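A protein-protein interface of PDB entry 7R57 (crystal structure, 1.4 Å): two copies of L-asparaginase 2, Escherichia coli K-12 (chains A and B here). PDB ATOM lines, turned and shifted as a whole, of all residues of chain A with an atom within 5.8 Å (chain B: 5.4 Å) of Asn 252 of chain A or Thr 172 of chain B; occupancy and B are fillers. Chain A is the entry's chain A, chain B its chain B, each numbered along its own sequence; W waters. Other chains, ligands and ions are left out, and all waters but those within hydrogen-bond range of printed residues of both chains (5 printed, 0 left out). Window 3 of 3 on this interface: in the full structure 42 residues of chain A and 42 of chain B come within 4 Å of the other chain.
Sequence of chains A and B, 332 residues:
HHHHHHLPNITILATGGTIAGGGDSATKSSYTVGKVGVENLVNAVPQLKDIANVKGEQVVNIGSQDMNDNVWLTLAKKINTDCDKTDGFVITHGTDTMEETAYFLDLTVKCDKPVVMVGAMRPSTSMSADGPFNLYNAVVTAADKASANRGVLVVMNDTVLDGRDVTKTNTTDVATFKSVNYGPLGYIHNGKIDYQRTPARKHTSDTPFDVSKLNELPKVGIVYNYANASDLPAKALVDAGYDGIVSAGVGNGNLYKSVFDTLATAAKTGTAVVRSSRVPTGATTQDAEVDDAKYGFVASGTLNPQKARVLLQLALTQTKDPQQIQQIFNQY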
ATOM      1  N   VAL A 250      17.036   4.619  -1.611  1.00  0.00           N
ATOM      2  CA  VAL A 250      16.120   3.542  -1.243  1.00  0.00           C
ATOM      3  C   VAL A 250      14.705   3.995  -1.559  1.00  0.00           C
ATOM      4  O   VAL A 250      14.363   5.178  -1.465  1.00  0.00           O
ATOM      5  CB  VAL A 250      16.279   3.133   0.243  1.00  0.00           C
ATOM      6  CG1 VAL A 250      17.672   2.572   0.491  1.00  0.00           C
ATOM      7  CG2 VAL A 250      16.028   4.292   1.211  1.00  0.00           C
ATOM      8  N   GLY A 251      13.873   3.040  -1.984  1.00  0.00           N
ATOM      9  CA  GLY A 251      12.521   3.402  -2.335  1.00  0.00           C
ATOM     10  C   GLY A 251      12.500   4.477  -3.404  1.00  0.00           C
ATOM     11  O   GLY A 251      13.242   4.439  -4.403  1.00  0.00           O
ATOM     12  N   ASN A 252      11.591   5.440  -3.233  1.00  0.00           N
ATOM     13  CA  ASN A 252      11.440   6.556  -4.170  1.00  0.00           C
ATOM     14  C   ASN A 252      12.536   7.599  -3.936  1.00  0.00           C
ATOM     15  O   ASN A 252      12.268   8.743  -3.575  1.00  0.00           O
ATOM     16  CB  ASN A 252      10.040   7.139  -4.034  1.00  0.00           C
ATOM     17  CG  ASN A 252       9.650   8.068  -5.171  1.00  0.00           C
ATOM     18  OD1 ASN A 252      10.467   8.462  -6.006  1.00  0.00           O
ATOM     19  ND2 ASN A 252       8.384   8.448  -5.178  1.00  0.00           N
ATOM     20  N   GLY A 253      13.783   7.176  -4.149  1.00  0.00           N
ATOM     21  CA  GLY A 253      14.911   8.093  -4.077  1.00  0.00           C
ATOM     22  C   GLY A 253      15.271   8.643  -2.712  1.00  0.00           C
ATOM     23  O   GLY A 253      15.883   9.717  -2.644  1.00  0.00           O
ATOM     24  N   ASN A 254      14.953   7.950  -1.635  1.00  0.00           N
ATOM     25  CA  ASN A 254      15.247   8.428  -0.288  1.00  0.00           C
ATOM     26  C   ASN A 254      16.699   8.123   0.060  1.00  0.00           C
ATOM     27  O   ASN A 254      17.358   7.253  -0.521  1.00  0.00           O
ATOM     28  CB  ASN A 254      14.259   7.823   0.709  1.00  0.00           C
ATOM     29  CG  ASN A 254      12.881   8.405   0.584  1.00  0.00           C
ATOM     30  OD1 ASN A 254      12.723   9.611   0.360  1.00  0.00           O
ATOM     31  ND2 ASN A 254      11.863   7.564   0.683  1.00  0.00           N
ATOM     32  N   ARG A 275      19.016  12.589  -7.203  1.00  0.00           N
ATOM     33  CA  ARG A 275      18.393  11.462  -6.511  1.00  0.00           C
ATOM     34  C   ARG A 275      17.888  10.468  -7.559  1.00  0.00           C
ATOM     35  O   ARG A 275      16.940  10.767  -8.298  1.00  0.00           O
ATOM     36  CB  ARG A 275      17.211  11.903  -5.655  1.00  0.00           C
ATOM     37  CG  ARG A 275      17.604  12.859  -4.566  1.00  0.00           C
ATOM     38  CD  ARG A 275      16.470  13.061  -3.553  1.00  0.00           C
ATOM     39  NE  ARG A 275      15.243  13.518  -4.186  1.00  0.00           N
ATOM     40  CZ  ARG A 275      14.135  12.806  -4.377  1.00  0.00           C
ATOM     41  NH1 ARG A 275      14.029  11.543  -3.967  1.00  0.00           N
ATOM     42  NH2 ARG A 275      13.117  13.363  -5.020  1.00  0.00           N
ATOM     43  N   SER A 276      18.487   9.273  -7.582  1.00  0.00           N
ATOM     44  CA  SER A 276      17.990   8.112  -8.294  1.00  0.00           C
ATOM     45  C   SER A 276      17.605   7.066  -7.249  1.00  0.00           C
ATOM     46  O   SER A 276      17.466   7.371  -6.041  1.00  0.00           O
ATOM     47  CB  SER A 276      19.037   7.633  -9.304  1.00  0.00           C
ATOM     48  OG  SER A 276      18.622   6.502 -10.064  1.00  0.00           O
ATOM     49  N   SER A 277      17.488   5.824  -7.684  1.00  0.00           N
ATOM     50  CA  SER A 277      17.063   4.744  -6.803  1.00  0.00           C
ATOM     51  C   SER A 277      17.767   3.443  -7.130  1.00  0.00           C
ATOM     52  O   SER A 277      17.911   3.088  -8.288  1.00  0.00           O
ATOM     53  CB  SER A 277      15.545   4.531  -6.818  1.00  0.00           C
ATOM     54  OG  SER A 277      15.230   3.480  -5.920  1.00  0.00           O
ATOM     55  N   VAL A 279      16.245   0.822  -6.580  1.00  0.00           N
ATOM     56  CA  VAL A 279      15.091  -0.005  -6.936  1.00  0.00           C
ATOM     57  C   VAL A 279      15.055  -0.132  -8.452  1.00  0.00           C
ATOM     58  O   VAL A 279      15.206   0.878  -9.155  1.00  0.00           O
ATOM     59  CB  VAL A 279      13.829   0.623  -6.374  1.00  0.00           C
ATOM     60  CG1 VAL A 279      12.643  -0.188  -6.829  1.00  0.00           C
ATOM     61  CG2 VAL A 279      13.860   0.673  -4.854  1.00  0.00           C
ATOM     62  N   THR A 281      13.022  -0.726 -11.015  1.00  0.00           N
ATOM     63  CA  THR A 281      12.007  -0.213 -11.934  1.00  0.00           C
ATOM     64  C   THR A 281      11.279   0.938 -11.251  1.00  0.00           C
ATOM     65  O   THR A 281      11.239   1.034 -10.026  1.00  0.00           O
ATOM     66  CB  THR A 281      10.984  -1.300 -12.394  1.00  0.00           C
ATOM     67  OG1 THR A 281      10.077  -1.584 -11.322  1.00  0.00           O
ATOM     68  CG2 THR A 281      11.640  -2.576 -12.900  1.00  0.00           C
ATOM     69  N   GLY A 282      10.696   1.813 -12.059  1.00  0.00           N
ATOM     70  CA  GLY A 282       9.932   2.915 -11.533  1.00  0.00           C
ATOM     71  C   GLY A 282      10.732   4.205 -11.459  1.00  0.00           C
ATOM     72  O   GLY A 282      11.967   4.219 -11.370  1.00  0.00           O
ATOM     73  N   ALA A 283      10.007   5.310 -11.416  1.00  0.00           N
ATOM     74  CA  ALA A 283      10.643   6.618 -11.348  1.00  0.00           C
ATOM     75  C   ALA A 283      10.967   7.044  -9.918  1.00  0.00           C
ATOM     76  O   ALA A 283      10.217   6.770  -8.967  1.00  0.00           O
ATOM     77  CB  ALA A 283       9.718   7.662 -11.989  1.00  0.00           C
ATOM     78  N   THR A 284      12.081   7.777  -9.782  1.00  0.00           N
ATOM     79  CA  THR A 284      12.321   8.648  -8.631  1.00  0.00           C
ATOM     80  C   THR A 284      11.635   9.967  -8.959  1.00  0.00           C
ATOM     81  O   THR A 284      12.081  10.699  -9.848  1.00  0.00           O
ATOM     82  CB  THR A 284      13.807   8.830  -8.341  1.00  0.00           C
ATOM     83  OG1 THR A 284      14.353   7.562  -7.947  1.00  0.00           O
ATOM     84  CG2 THR A 284      14.006   9.824  -7.193  1.00  0.00           C
ATOM     85  N   THR A 285      10.552  10.255  -8.256  1.00  0.00           N
ATOM     86  CA  THR A 285       9.652  11.334  -8.612  1.00  0.00           C
ATOM     87  C   THR A 285       9.965  12.618  -7.869  1.00  0.00           C
ATOM     88  O   THR A 285      10.561  12.635  -6.795  1.00  0.00           O
ATOM     89  CB  THR A 285       8.186  10.933  -8.363  1.00  0.00           C
ATOM     90  OG1 THR A 285       7.955  10.780  -6.955  1.00  0.00           O
ATOM     91  CG2 THR A 285       7.819   9.649  -9.090  1.00  0.00           C
ATOM     92  N   ALA A 288       7.625  13.893  -3.703  1.00  0.00           N
ATOM     93  CA  ALA A 288       7.449  12.690  -2.840  1.00  0.00           C
ATOM     94  C   ALA A 288       7.940  13.086  -1.457  1.00  0.00           C
ATOM     95  O   ALA A 288       7.477  14.083  -0.914  1.00  0.00           O
ATOM     96  CB  ALA A 288       8.080  11.470  -3.482  1.00  0.00           C
ATOM     97  N   GLU A 289       8.893  12.332  -0.867  1.00  0.00           N
ATOM     98  CA  GLU A 289       9.332  12.620   0.495  1.00  0.00           C
ATOM     99  C   GLU A 289      10.437  13.666   0.580  1.00  0.00           C
ATOM    100  O   GLU A 289      10.676  14.191   1.675  1.00  0.00           O
ATOM    101  CB  GLU A 289       9.841  11.360   1.207  1.00  0.00           C
ATOM    102  CG  GLU A 289       8.790  10.550   1.939  1.00  0.00           C
ATOM    103  CD  GLU A 289       9.372   9.279   2.559  1.00  0.00           C
ATOM    104  OE1 GLU A 289       9.974   9.361   3.655  1.00  0.00           O
ATOM    105  OE2 GLU A 289       9.244   8.203   1.938  1.00  0.00           O
ATOM    106  N   VAL A 290      11.108  14.002  -0.524  1.00  0.00           N
ATOM    107  CA  VAL A 290      12.223  14.934  -0.491  1.00  0.00           C
ATOM    108  C   VAL A 290      11.833  16.218  -1.208  1.00  0.00           C
ATOM    109  O   VAL A 290      11.441  16.192  -2.381  1.00  0.00           O
ATOM    110  CB  VAL A 290      13.497  14.327  -1.097  1.00  0.00           C
ATOM    111  CG1 VAL A 290      14.628  15.350  -1.049  1.00  0.00           C
ATOM    112  CG2 VAL A 290      13.866  13.048  -0.362  1.00  0.00           C
ATOM    113  N   ASP B  96      11.153   1.062   2.334  1.00  0.00           N
ATOM    114  CA  ASP B  96      12.419   1.311   1.653  1.00  0.00           C
ATOM    115  C   ASP B  96      13.489   0.287   2.028  1.00  0.00           C
ATOM    116  O   ASP B  96      14.261  -0.139   1.169  1.00  0.00           O
ATOM    117  CB  ASP B  96      12.928   2.707   1.978  1.00  0.00           C
ATOM    118  CG  ASP B  96      12.093   3.776   1.361  1.00  0.00           C
ATOM    119  OD1 ASP B  96      11.187   3.445   0.594  1.00  0.00           O
ATOM    120  OD2 ASP B  96      12.352   4.980   1.615  1.00  0.00           O
ATOM    121  N   MET B 121       2.646   1.067   0.659  1.00  0.00           N
ATOM    122  CA  MET B 121       3.205   1.918  -0.379  1.00  0.00           C
ATOM    123  C   MET B 121       2.426   3.203  -0.575  1.00  0.00           C
ATOM    124  O   MET B 121       2.939   4.119  -1.223  1.00  0.00           O
ATOM    125  CB  MET B 121       3.249   1.135  -1.681  1.00  0.00           C
ATOM    126  CG  MET B 121       4.280   0.060  -1.674  1.00  0.00           C
ATOM    127  SD  MET B 121       5.974   0.704  -1.578  1.00  0.00           S
ATOM    128  CE  MET B 121       6.160   1.320  -3.226  1.00  0.00           C
ATOM    129  N   LYS B 168      12.254  -5.016  -3.003  1.00  0.00           N
ATOM    130  CA  LYS B 168      11.403  -3.974  -3.530  1.00  0.00           C
ATOM    131  C   LYS B 168      11.799  -3.748  -4.982  1.00  0.00           C
ATOM    132  O   LYS B 168      12.905  -3.284  -5.261  1.00  0.00           O
ATOM    133  CB  LYS B 168      11.587  -2.712  -2.670  1.00  0.00           C
ATOM    134  CG  LYS B 168      10.684  -1.566  -3.038  1.00  0.00           C
ATOM    135  CD  LYS B 168      10.726  -0.407  -1.998  1.00  0.00           C
ATOM    136  CE  LYS B 168       9.695   0.644  -2.317  1.00  0.00           C
ATOM    137  NZ  LYS B 168       9.560   1.691  -1.244  1.00  0.00           N
ATOM    138  N   ASN B 170       9.904  -1.954  -7.461  1.00  0.00           N
ATOM    139  CA  ASN B 170       9.379  -0.740  -8.081  1.00  0.00           C
ATOM    140  C   ASN B 170       9.273   0.385  -7.058  1.00  0.00           C
ATOM    141  O   ASN B 170       8.919   0.163  -5.900  1.00  0.00           O
ATOM    142  CB  ASN B 170       8.003  -1.011  -8.722  1.00  0.00           C
ATOM    143  CG  ASN B 170       7.492   0.163  -9.503  1.00  0.00           C
ATOM    144  OD1 ASN B 170       6.792   1.033  -8.971  1.00  0.00           O
ATOM    145  ND2 ASN B 170       7.852   0.218 -10.771  1.00  0.00           N
ATOM    146  N   THR B 171       9.527   1.613  -7.510  1.00  0.00           N
ATOM    147  CA  THR B 171       9.588   2.704  -6.559  1.00  0.00           C
ATOM    148  C   THR B 171       8.238   3.112  -5.973  1.00  0.00           C
ATOM    149  O   THR B 171       8.229   3.713  -4.891  1.00  0.00           O
ATOM    150  CB  THR B 171      10.172   3.950  -7.243  1.00  0.00           C
ATOM    151  OG1 THR B 171       9.436   4.172  -8.436  1.00  0.00           O
ATOM    152  CG2 THR B 171      11.654   3.789  -7.571  1.00  0.00           C
ATOM    153  N   THR B 172       7.115   2.843  -6.658  1.00  0.00           N
ATOM    154  CA  THR B 172       5.799   3.333  -6.248  1.00  0.00           C
ATOM    155  C   THR B 172       4.672   2.293  -6.233  1.00  0.00           C
ATOM    156  O   THR B 172       3.662   2.519  -5.553  1.00  0.00           O
ATOM    157  CB  THR B 172       5.356   4.511  -7.129  1.00  0.00           C
ATOM    158  OG1 THR B 172       5.334   4.129  -8.499  1.00  0.00           O
ATOM    159  CG2 THR B 172       6.315   5.681  -6.986  1.00  0.00           C
ATOM    160  N   ASP B 173       4.813   1.155  -6.908  1.00  0.00           N
ATOM    161  CA  ASP B 173       3.696   0.238  -7.114  1.00  0.00           C
ATOM    162  C   ASP B 173       3.353  -0.480  -5.822  1.00  0.00           C
ATOM    163  O   ASP B 173       4.234  -0.999  -5.127  1.00  0.00           O
ATOM    164  CB  ASP B 173       4.163  -0.786  -8.152  1.00  0.00           C
ATOM    165  CG  ASP B 173       3.078  -1.679  -8.718  1.00  0.00           C
ATOM    166  OD1 ASP B 173       2.021  -1.955  -8.124  1.00  0.00           O
ATOM    167  OD2 ASP B 173       3.364  -2.168  -9.857  1.00  0.00           O
ATOM    168  N   VAL B 174       2.050  -0.598  -5.543  1.00  0.00           N
ATOM    169  CA  VAL B 174       1.628  -1.394  -4.387  1.00  0.00           C
ATOM    170  C   VAL B 174       2.061  -2.861  -4.484  1.00  0.00           C
ATOM    171  O   VAL B 174       2.145  -3.534  -3.460  1.00  0.00           O
ATOM    172  CB  VAL B 174       0.102  -1.338  -4.149  1.00  0.00           C
ATOM    173  CG1 VAL B 174      -0.335   0.057  -3.808  1.00  0.00           C
ATOM    174  CG2 VAL B 174      -0.700  -1.871  -5.346  1.00  0.00           C
HETATM  175  O   HOH W   1      14.346   0.339  -1.450  1.00  0.00           O
HETATM  176  O   HOH W   2       9.967   5.391  -0.871  1.00  0.00           O
HETATM  177  O   HOH W   3       7.156   4.742 -10.465  1.00  0.00           O
HETATM  178  O   HOH W   4      10.957   6.097   3.427  1.00  0.00           O
HETATM  179  O   HOH W   5       7.984   0.833 -13.892  1.00  0.00           O
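The side-chain hydroxyl (OG1) of Thr 281 of chain A lies within hydrogen-bond range of the side-chain amide nitrogen (ND2) of Asn 170 of chain B (2.9 Å).
O of Thr 281 of chain A sits at hydrogen-bond distance from N of Thr 171 of chain B, at 3.1 Å.
ND2 of Asn 254 of chain A sits at hydrogen-bond distance from OD2 of Asp 96 of chain B (2.8 Å).
The backbone carbonyl oxygen (O) of Ala 283 of chain A is in hydrogen-bond range of the side-chain hydroxyl (OG1) of Thr 171 of chain B.
The backbone carbonyl oxygen (O) of Gly 251 of chain A lies within hydrogen-bond range of the side-chain hydroxyl (OG) of Ser 277 of chain A (2.7 Å).
The backbone NH (N) of Val 279 of chain A is in hydrogen-bond range of the side-chain hydroxyl (OG) of Ser 277 of chain A (2.9 Å).
The side-chain amide oxygen of Asn 170 of chain B lies within hydrogen-bond range of the backbone NH of Asp 173 of chain B.
The side-chain carboxylate (OD1) of Asp 96 of chain B is in salt-bridge range of the side-chain amino group (NZ) of Lys 168 of chain B (3.0 Å).
NH1 of Arg 275 of chain A is in hydrogen-bond range of O of Asn 252 of chain A (3.3 Å).
The backbone carbonyl oxygen of Ala 283 of chain A sits close to the side-chain amide oxygen of Asn 252 of chain A (3.4 Å).
Among the printed residues, pairs that only touch across the chains: Val 250 of chain A with Asp 96 of chain B, Gly 251 of chain A with Asp 96 of chain B, Gly 251 of chain A with Lys 168 of chain B, Gly 251 of chain A with Thr 171 of chain B, Asn 252 of chain A with Thr 171 of chain B, Asn 252 of chain A with Thr 172 of chain B, Ser 277 of chain A with Thr 171 of chain B, Val 279 of chain A with Lys 168 of chain B, Val 279 of chain A with Asn 170 of chain B, Val 279 of chain A with Thr 171 of chain B, Gly 282 of chain A with Asn 170 of chain B and Gly 282 of chain A with Thr 171 of chain B.
Of chain B, only Thr 171 and Thr 172 come within 4 Å of Asn 252 of chain A.
Thr 172 of chain B touches just one residue of chain A: Asn 252.
Of the printed residues of chain B, Val 279 of chain A touches Lys 168 (3.5 Å), Asn 170 (3.3 Å) and Thr 171 (3.7 Å).
Printed residues of chain B within 4 Å of Asn 254 of chain A: Asp 96.
Of the printed residues of chain B, Val 250 of chain A touches Asp 96 (3.6 Å).
Of the printed residues of chain B, Ser 277 of chain A touches Thr 171.
Of the 8 printed residues of chain B, 5 touch a printed residue of chain A.
Along chain B the printed residues that touch a printed residue of chain A span positions 96 to 172.
No position is printed for both chains.
Of the 16 pairs that touch across the chains among the printed residues, none has its exchanged pair printed and touching as well.
Water W4 lies within hydrogen-bond range of OD2 of Asp 96 of chain B (2.5 Å), OE2 of Glu 289 of chain A (3.1 Å) and ND2 of Asn 254 of chain A (3.2 Å).
Water W1 bridges the backbone carbonyl oxygen of Asp 96 of chain B (2.7 Å) and the backbone NH of Gly 251 of chain A (2.8 Å).
Water W2 lies within hydrogen-bond range of the side-chain carboxylate of Asp 96 of chain B (2.7 Å), the backbone NH of Asn 252 of chain A (2.9 Å) and the side-chain amide nitrogen of Asn 254 of chain A (3.3 Å).
Water W3 lies within hydrogen-bond range of OG1 of Thr 172 of chain B (2.7 Å), N of Ala 283 of chain A (3.1 Å) and OG1 of Thr 171 of chain B (3.1 Å).
Water W5 bridges the side-chain amide nitrogen (ND2) of Asn 170 of chain B and the backbone NH (N) of Gly 282 of chain A.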
